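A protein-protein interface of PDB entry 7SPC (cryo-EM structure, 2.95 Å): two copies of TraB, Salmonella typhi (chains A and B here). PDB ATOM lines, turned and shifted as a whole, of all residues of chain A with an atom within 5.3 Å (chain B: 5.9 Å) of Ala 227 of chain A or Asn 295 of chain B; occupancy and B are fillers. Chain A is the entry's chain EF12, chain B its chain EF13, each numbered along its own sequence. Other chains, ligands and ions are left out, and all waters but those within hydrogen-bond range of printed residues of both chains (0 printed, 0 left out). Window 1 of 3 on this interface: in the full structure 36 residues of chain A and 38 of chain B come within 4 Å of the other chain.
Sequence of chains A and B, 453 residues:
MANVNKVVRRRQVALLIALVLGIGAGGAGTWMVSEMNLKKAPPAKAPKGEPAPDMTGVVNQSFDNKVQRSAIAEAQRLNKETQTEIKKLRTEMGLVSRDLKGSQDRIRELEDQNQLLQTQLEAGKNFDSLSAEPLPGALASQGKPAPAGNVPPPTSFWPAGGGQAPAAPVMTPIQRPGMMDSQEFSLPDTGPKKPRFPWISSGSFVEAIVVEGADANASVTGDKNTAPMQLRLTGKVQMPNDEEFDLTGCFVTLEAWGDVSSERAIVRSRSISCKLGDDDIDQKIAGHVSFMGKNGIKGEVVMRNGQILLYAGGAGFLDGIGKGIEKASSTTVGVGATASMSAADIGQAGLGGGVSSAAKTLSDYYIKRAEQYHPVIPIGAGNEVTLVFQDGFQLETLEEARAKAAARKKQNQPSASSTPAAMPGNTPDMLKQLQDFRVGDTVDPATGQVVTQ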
ATOM      1  N   GLU A 212     -15.977 -11.806  13.376  1.00  0.00           N
ATOM      2  CA  GLU A 212     -16.545 -12.584  12.284  1.00  0.00           C
ATOM      3  C   GLU A 212     -17.322 -11.645  11.373  1.00  0.00           C
ATOM      4  O   GLU A 212     -18.198 -10.912  11.839  1.00  0.00           O
ATOM      5  CB  GLU A 212     -17.447 -13.697  12.822  1.00  0.00           C
ATOM      6  CG  GLU A 212     -18.167 -14.497  11.752  1.00  0.00           C
ATOM      7  CD  GLU A 212     -19.367 -15.245  12.298  1.00  0.00           C
ATOM      8  OE1 GLU A 212     -19.851 -16.172  11.617  1.00  0.00           O
ATOM      9  OE2 GLU A 212     -19.826 -14.910  13.411  1.00  0.00           O
ATOM     10  N   GLY A 213     -16.987 -11.653  10.083  1.00  0.00           N
ATOM     11  CA  GLY A 213     -17.693 -10.875   9.093  1.00  0.00           C
ATOM     12  C   GLY A 213     -18.733 -11.698   8.357  1.00  0.00           C
ATOM     13  O   GLY A 213     -19.089 -12.807   8.756  1.00  0.00           O
ATOM     14  N   ALA A 214     -19.223 -11.135   7.254  1.00  0.00           N
ATOM     15  CA  ALA A 214     -20.194 -11.811   6.398  1.00  0.00           C
ATOM     16  C   ALA A 214     -20.439 -10.955   5.164  1.00  0.00           C
ATOM     17  O   ALA A 214     -20.028  -9.794   5.093  1.00  0.00           O
ATOM     18  CB  ALA A 214     -21.520 -12.075   7.110  1.00  0.00           C
ATOM     19  N   ASP A 215     -21.113 -11.553   4.186  1.00  0.00           N
ATOM     20  CA  ASP A 215     -21.707 -10.834   3.069  1.00  0.00           C
ATOM     21  C   ASP A 215     -23.175 -10.600   3.392  1.00  0.00           C
ATOM     22  O   ASP A 215     -23.913 -11.552   3.657  1.00  0.00           O
ATOM     23  CB  ASP A 215     -21.557 -11.611   1.763  1.00  0.00           C
ATOM     24  CG  ASP A 215     -20.118 -11.986   1.473  1.00  0.00           C
ATOM     25  OD1 ASP A 215     -19.523 -12.736   2.271  1.00  0.00           O
ATOM     26  OD2 ASP A 215     -19.584 -11.530   0.442  1.00  0.00           O
ATOM     27  N   ASN A 225     -33.339 -12.725   5.586  1.00  0.00           N
ATOM     28  CA  ASN A 225     -32.196 -13.614   5.391  1.00  0.00           C
ATOM     29  C   ASN A 225     -30.961 -12.898   5.932  1.00  0.00           C
ATOM     30  O   ASN A 225     -30.286 -12.160   5.217  1.00  0.00           O
ATOM     31  CB  ASN A 225     -32.036 -13.978   3.922  1.00  0.00           C
ATOM     32  CG  ASN A 225     -33.359 -14.265   3.245  1.00  0.00           C
ATOM     33  OD1 ASN A 225     -34.237 -14.904   3.821  1.00  0.00           O
ATOM     34  ND2 ASN A 225     -33.509 -13.792   2.014  1.00  0.00           N
ATOM     35  N   THR A 226     -30.664 -13.129   7.206  1.00  0.00           N
ATOM     36  CA  THR A 226     -29.569 -12.462   7.893  1.00  0.00           C
ATOM     37  C   THR A 226     -28.414 -13.431   8.122  1.00  0.00           C
ATOM     38  O   THR A 226     -28.570 -14.651   8.033  1.00  0.00           O
ATOM     39  CB  THR A 226     -30.036 -11.881   9.233  1.00  0.00           C
ATOM     40  OG1 THR A 226     -30.836 -12.850   9.921  1.00  0.00           O
ATOM     41  CG2 THR A 226     -30.866 -10.634   9.004  1.00  0.00           C
ATOM     42  N   ALA A 227     -27.249 -12.866   8.422  1.00  0.00           N
ATOM     43  CA  ALA A 227     -26.028 -13.626   8.625  1.00  0.00           C
ATOM     44  C   ALA A 227     -25.350 -13.204   9.918  1.00  0.00           C
ATOM     45  O   ALA A 227     -25.414 -12.034  10.303  1.00  0.00           O
ATOM     46  CB  ALA A 227     -25.060 -13.428   7.450  1.00  0.00           C
ATOM     47  N   PRO A 228     -24.687 -14.133  10.606  1.00  0.00           N
ATOM     48  CA  PRO A 228     -24.028 -13.790  11.872  1.00  0.00           C
ATOM     49  C   PRO A 228     -22.700 -13.081  11.652  1.00  0.00           C
ATOM     50  O   PRO A 228     -21.888 -13.488  10.815  1.00  0.00           O
ATOM     51  CB  PRO A 228     -23.819 -15.157  12.540  1.00  0.00           C
ATOM     52  CG  PRO A 228     -24.677 -16.116  11.762  1.00  0.00           C
ATOM     53  CD  PRO A 228     -24.694 -15.586  10.378  1.00  0.00           C
ATOM     54  N   MET A 229     -22.513 -11.987  12.393  1.00  0.00           N
ATOM     55  CA  MET A 229     -21.297 -11.150  12.233  1.00  0.00           C
ATOM     56  C   MET A 229     -20.836 -10.717  13.629  1.00  0.00           C
ATOM     57  O   MET A 229     -20.652  -9.505  13.837  1.00  0.00           O
ATOM     58  CB  MET A 229     -21.660  -9.918  11.394  1.00  0.00           C
ATOM     59  CG  MET A 229     -20.486  -9.203  10.753  1.00  0.00           C
ATOM     60  SD  MET A 229     -20.987  -7.735   9.821  1.00  0.00           S
ATOM     61  CE  MET A 229     -21.787  -8.500   8.415  1.00  0.00           C
ATOM     62  N   LEU A 254     -24.311 -10.922  16.700  1.00  0.00           N
ATOM     63  CA  LEU A 254     -25.182 -10.049  15.932  1.00  0.00           C
ATOM     64  C   LEU A 254     -25.702 -10.786  14.703  1.00  0.00           C
ATOM     65  O   LEU A 254     -25.312 -11.921  14.417  1.00  0.00           O
ATOM     66  CB  LEU A 254     -24.447  -8.779  15.488  1.00  0.00           C
ATOM     67  CG  LEU A 254     -24.364  -7.584  16.437  1.00  0.00           C
ATOM     68  CD1 LEU A 254     -23.530  -7.946  17.641  1.00  0.00           C
ATOM     69  CD2 LEU A 254     -23.774  -6.382  15.737  1.00  0.00           C
ATOM     70  N   GLU A 255     -26.594 -10.121  13.974  1.00  0.00           N
ATOM     71  CA  GLU A 255     -27.038 -10.575  12.664  1.00  0.00           C
ATOM     72  C   GLU A 255     -27.231  -9.357  11.772  1.00  0.00           C
ATOM     73  O   GLU A 255     -27.729  -8.324  12.222  1.00  0.00           O
ATOM     74  CB  GLU A 255     -28.329 -11.405  12.744  1.00  0.00           C
ATOM     75  CG  GLU A 255     -29.571 -10.636  13.144  1.00  0.00           C
ATOM     76  CD  GLU A 255     -30.608 -11.525  13.796  1.00  0.00           C
ATOM     77  OE1 GLU A 255     -30.264 -12.664  14.168  1.00  0.00           O
ATOM     78  OE2 GLU A 255     -31.767 -11.087  13.938  1.00  0.00           O
ATOM     79  N   ALA A 256     -26.821  -9.476  10.511  1.00  0.00           N
ATOM     80  CA  ALA A 256     -26.734  -8.326   9.630  1.00  0.00           C
ATOM     81  C   ALA A 256     -27.350  -8.619   8.270  1.00  0.00           C
ATOM     82  O   ALA A 256     -27.306  -9.745   7.773  1.00  0.00           O
ATOM     83  CB  ALA A 256     -25.283  -7.883   9.437  1.00  0.00           C
ATOM     84  N   ARG B 264     -20.635 -18.867  -1.461  1.00  0.00           N
ATOM     85  CA  ARG B 264     -20.197 -19.498  -0.227  1.00  0.00           C
ATOM     86  C   ARG B 264     -21.166 -20.594   0.184  1.00  0.00           C
ATOM     87  O   ARG B 264     -22.346 -20.576  -0.179  1.00  0.00           O
ATOM     88  CB  ARG B 264     -20.068 -18.475   0.910  1.00  0.00           C
ATOM     89  CG  ARG B 264     -18.963 -17.452   0.714  1.00  0.00           C
ATOM     90  CD  ARG B 264     -18.602 -16.777   2.019  1.00  0.00           C
ATOM     91  NE  ARG B 264     -17.231 -16.281   2.015  1.00  0.00           N
ATOM     92  CZ  ARG B 264     -16.356 -16.500   2.983  1.00  0.00           C
ATOM     93  NH1 ARG B 264     -16.674 -17.203   4.057  1.00  0.00           N
ATOM     94  NH2 ARG B 264     -15.128 -16.003   2.872  1.00  0.00           N
ATOM     95  N   ALA B 265     -20.656 -21.543   0.963  1.00  0.00           N
ATOM     96  CA  ALA B 265     -21.467 -22.629   1.500  1.00  0.00           C
ATOM     97  C   ALA B 265     -21.928 -22.251   2.902  1.00  0.00           C
ATOM     98  O   ALA B 265     -21.119 -22.175   3.832  1.00  0.00           O
ATOM     99  CB  ALA B 265     -20.677 -23.934   1.515  1.00  0.00           C
ATOM    100  N   ILE B 266     -23.225 -22.014   3.054  1.00  0.00           N
ATOM    101  CA  ILE B 266     -23.802 -21.716   4.359  1.00  0.00           C
ATOM    102  C   ILE B 266     -24.064 -23.037   5.068  1.00  0.00           C
ATOM    103  O   ILE B 266     -24.812 -23.884   4.569  1.00  0.00           O
ATOM    104  CB  ILE B 266     -25.087 -20.889   4.227  1.00  0.00           C
ATOM    105  CG1 ILE B 266     -24.870 -19.716   3.272  1.00  0.00           C
ATOM    106  CG2 ILE B 266     -25.530 -20.387   5.586  1.00  0.00           C
ATOM    107  CD1 ILE B 266     -23.752 -18.788   3.683  1.00  0.00           C
ATOM    108  N   HIS B 288     -22.590 -22.239  13.609  1.00  0.00           N
ATOM    109  CA  HIS B 288     -22.310 -22.110  12.186  1.00  0.00           C
ATOM    110  C   HIS B 288     -20.807 -22.207  11.973  1.00  0.00           C
ATOM    111  O   HIS B 288     -20.041 -22.464  12.904  1.00  0.00           O
ATOM    112  CB  HIS B 288     -22.880 -20.804  11.625  1.00  0.00           C
ATOM    113  CG  HIS B 288     -22.463 -19.584  12.383  1.00  0.00           C
ATOM    114  ND1 HIS B 288     -23.064 -19.200  13.561  1.00  0.00           N
ATOM    115  CD2 HIS B 288     -21.508 -18.659  12.130  1.00  0.00           C
ATOM    116  CE1 HIS B 288     -22.496 -18.094  14.003  1.00  0.00           C
ATOM    117  NE2 HIS B 288     -21.548 -17.747  13.152  1.00  0.00           N
ATOM    118  N   VAL B 289     -20.385 -22.005  10.729  1.00  0.00           N
ATOM    119  CA  VAL B 289     -18.994 -22.176  10.331  1.00  0.00           C
ATOM    120  C   VAL B 289     -18.516 -20.908   9.640  1.00  0.00           C
ATOM    121  O   VAL B 289     -19.216 -20.349   8.788  1.00  0.00           O
ATOM    122  CB  VAL B 289     -18.815 -23.404   9.413  1.00  0.00           C
ATOM    123  CG1 VAL B 289     -17.403 -23.469   8.867  1.00  0.00           C
ATOM    124  CG2 VAL B 289     -19.147 -24.680  10.166  1.00  0.00           C
ATOM    125  N   SER B 290     -17.325 -20.454  10.014  1.00  0.00           N
ATOM    126  CA  SER B 290     -16.667 -19.313   9.409  1.00  0.00           C
ATOM    127  C   SER B 290     -15.392 -19.762   8.711  1.00  0.00           C
ATOM    128  O   SER B 290     -14.710 -20.688   9.160  1.00  0.00           O
ATOM    129  CB  SER B 290     -16.335 -18.241  10.454  1.00  0.00           C
ATOM    130  OG  SER B 290     -17.398 -17.321  10.601  1.00  0.00           O
ATOM    131  N   PHE B 291     -15.079 -19.097   7.601  1.00  0.00           N
ATOM    132  CA  PHE B 291     -13.858 -19.361   6.850  1.00  0.00           C
ATOM    133  C   PHE B 291     -13.141 -18.040   6.619  1.00  0.00           C
ATOM    134  O   PHE B 291     -13.672 -17.159   5.937  1.00  0.00           O
ATOM    135  CB  PHE B 291     -14.164 -20.053   5.519  1.00  0.00           C
ATOM    136  CG  PHE B 291     -12.953 -20.260   4.658  1.00  0.00           C
ATOM    137  CD1 PHE B 291     -11.956 -21.135   5.044  1.00  0.00           C
ATOM    138  CD2 PHE B 291     -12.813 -19.575   3.464  1.00  0.00           C
ATOM    139  CE1 PHE B 291     -10.844 -21.322   4.256  1.00  0.00           C
ATOM    140  CE2 PHE B 291     -11.701 -19.761   2.676  1.00  0.00           C
ATOM    141  CZ  PHE B 291     -10.715 -20.637   3.073  1.00  0.00           C
ATOM    142  N   GLY B 293     -12.599 -15.635   8.690  1.00  0.00           N
ATOM    143  CA  GLY B 293     -13.220 -14.516   9.366  1.00  0.00           C
ATOM    144  C   GLY B 293     -14.567 -14.081   8.844  1.00  0.00           C
ATOM    145  O   GLY B 293     -15.099 -13.072   9.323  1.00  0.00           O
ATOM    146  N   LYS B 294     -15.145 -14.797   7.885  1.00  0.00           N
ATOM    147  CA  LYS B 294     -16.448 -14.448   7.343  1.00  0.00           C
ATOM    148  C   LYS B 294     -17.371 -15.652   7.417  1.00  0.00           C
ATOM    149  O   LYS B 294     -16.926 -16.801   7.376  1.00  0.00           O
ATOM    150  CB  LYS B 294     -16.347 -13.954   5.899  1.00  0.00           C
ATOM    151  CG  LYS B 294     -15.917 -12.506   5.774  1.00  0.00           C
ATOM    152  CD  LYS B 294     -15.326 -12.218   4.412  1.00  0.00           C
ATOM    153  CE  LYS B 294     -16.322 -11.505   3.524  1.00  0.00           C
ATOM    154  NZ  LYS B 294     -17.459 -12.387   3.154  1.00  0.00           N
ATOM    155  N   ASN B 295     -18.666 -15.373   7.539  1.00  0.00           N
ATOM    156  CA  ASN B 295     -19.659 -16.430   7.655  1.00  0.00           C
ATOM    157  C   ASN B 295     -19.677 -17.291   6.397  1.00  0.00           C
ATOM    158  O   ASN B 295     -19.642 -16.781   5.274  1.00  0.00           O
ATOM    159  CB  ASN B 295     -21.039 -15.822   7.898  1.00  0.00           C
ATOM    160  CG  ASN B 295     -22.071 -16.853   8.269  1.00  0.00           C
ATOM    161  OD1 ASN B 295     -21.795 -17.770   9.039  1.00  0.00           O
ATOM    162  ND2 ASN B 295     -23.272 -16.709   7.726  1.00  0.00           N
ATOM    163  N   GLY B 296     -19.728 -18.605   6.592  1.00  0.00           N
ATOM    164  CA  GLY B 296     -19.737 -19.542   5.493  1.00  0.00           C
ATOM    165  C   GLY B 296     -18.343 -19.854   4.982  1.00  0.00           C
ATOM    166  O   GLY B 296     -17.350 -19.229   5.351  1.00  0.00           O
ATOM    167  N   ILE B 297     -18.278 -20.844   4.097  1.00  0.00           N
ATOM    168  CA  ILE B 297     -17.023 -21.321   3.526  1.00  0.00           C
ATOM    169  C   ILE B 297     -16.963 -20.890   2.068  1.00  0.00           C
ATOM    170  O   ILE B 297     -17.943 -21.025   1.332  1.00  0.00           O
ATOM    171  CB  ILE B 297     -16.876 -22.848   3.653  1.00  0.00           C
ATOM    172  CG1 ILE B 297     -17.414 -23.327   4.997  1.00  0.00           C
ATOM    173  CG2 ILE B 297     -15.428 -23.254   3.512  1.00  0.00           C
ATOM    174  CD1 ILE B 297     -17.678 -24.808   5.043  1.00  0.00           C
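OE1 of Glu 212 of chain A sits at hydrogen-bond distance from NE2 of His 288 of chain B (2.8 Å).
OG of Ser 290 of chain B lies within hydrogen-bond range of OE1 of Glu 212 of chain A (2.9 Å).
N of Gly 213 of chain A lies within hydrogen-bond range of O of Gly 293 of chain B (2.5 Å).
The backbone carbonyl oxygen (O) of Gly 213 of chain A is in hydrogen-bond range of the backbone NH (N) of Asn 295 of chain B (2.9 Å).
OD2 of Asp 215 of chain A is in salt-bridge range of NZ of Lys 294 of chain B (3.6 Å).
The backbone carbonyl oxygen of Ala 227 of chain A sits at hydrogen-bond distance from the backbone NH of Ala 256 of chain A (2.9 Å).
NH1 of Arg 264 of chain B lies within hydrogen-bond range of O of Lys 294 of chain B (3.4 Å).
The guanidinium group of Arg 264 of chain B is in hydrogen-bond range of the backbone carbonyl oxygen of Asn 295 of chain B (3.2 Å).
OG of Ser 290 of chain B sits close to O of Lys 294 of chain B (3.3 Å).
Ala 227 of chain A touches just one residue of chain B: Asn 295 (3.7 Å).
Of the printed residues of chain A, Asn 295 of chain B touches Glu 212 (3.6 Å), Gly 213 (2.9 Å), Ala 214 (3.9 Å), Ala 227 (3.7 Å) and Pro 228 (3.2 Å).
Printed residues of chain B within 4 Å of Ala 214 of chain A: Lys 294 and Asn 295.
Printed residues of chain B within 4 Å of Glu 212 of chain A: His 288, Ser 290, Gly 293 and Asn 295.
Printed residues of chain B within 4 Å of Asp 215 of chain A: Lys 294 (2.3 Å).
Of the printed residues of chain A, Lys 294 of chain B touches Gly 213, Ala 214 and Asp 215.
Of the printed residues of chain A, Gly 293 of chain B touches Glu 212 (3.3 Å) and Gly 213 (2.5 Å).
Glu 255 of chain A touches none of the printed residues of chain B.
The nearest residue of chain A that does not touch Asn 295 of chain B is Asp 215 of chain A (5.0 Å).
The nearest printed residue of chain B that does not touch Gly 213 of chain A is Ser 290 of chain B (5.2 Å).
Of the 12 printed residues of chain A, 6 touch a printed residue of chain B.
Hydrophobic or aromatic side chains of chain A within 4 Å of the printed part of chain B: Ala 214, Ala 227 and Pro 228.
Hydrophobic or aromatic side chains of chain B that line the printed part of chain A: His 288.
Among the printed residues, 13 pairs touch across the chains.
O of Gly 293 of chain B touches CA of Glu 212 of chain A (3.3 Å).
OE1 of Glu 212 of chain A touches OD1 of Asn 295 of chain B, 3.6 Å away.
CA of Lys 294 of chain B touches O of Gly 213 of chain A, at 3.4 Å.
Ala 214 of chain A touches Lys 294 of chain B (C to NZ, 3.9 Å).
Ala 214 of chain A touches Asn 295 of chain B.
Asn 295 of chain B touches Ala 227 of chain A.
NE2 of His 288 of chain B touches CB of Pro 228 of chain A, 3.5 Å away.
Pro 228 of chain A touches Asn 295 of chain B (CD to ND2, 3.2 Å).
No position is printed for both chains.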
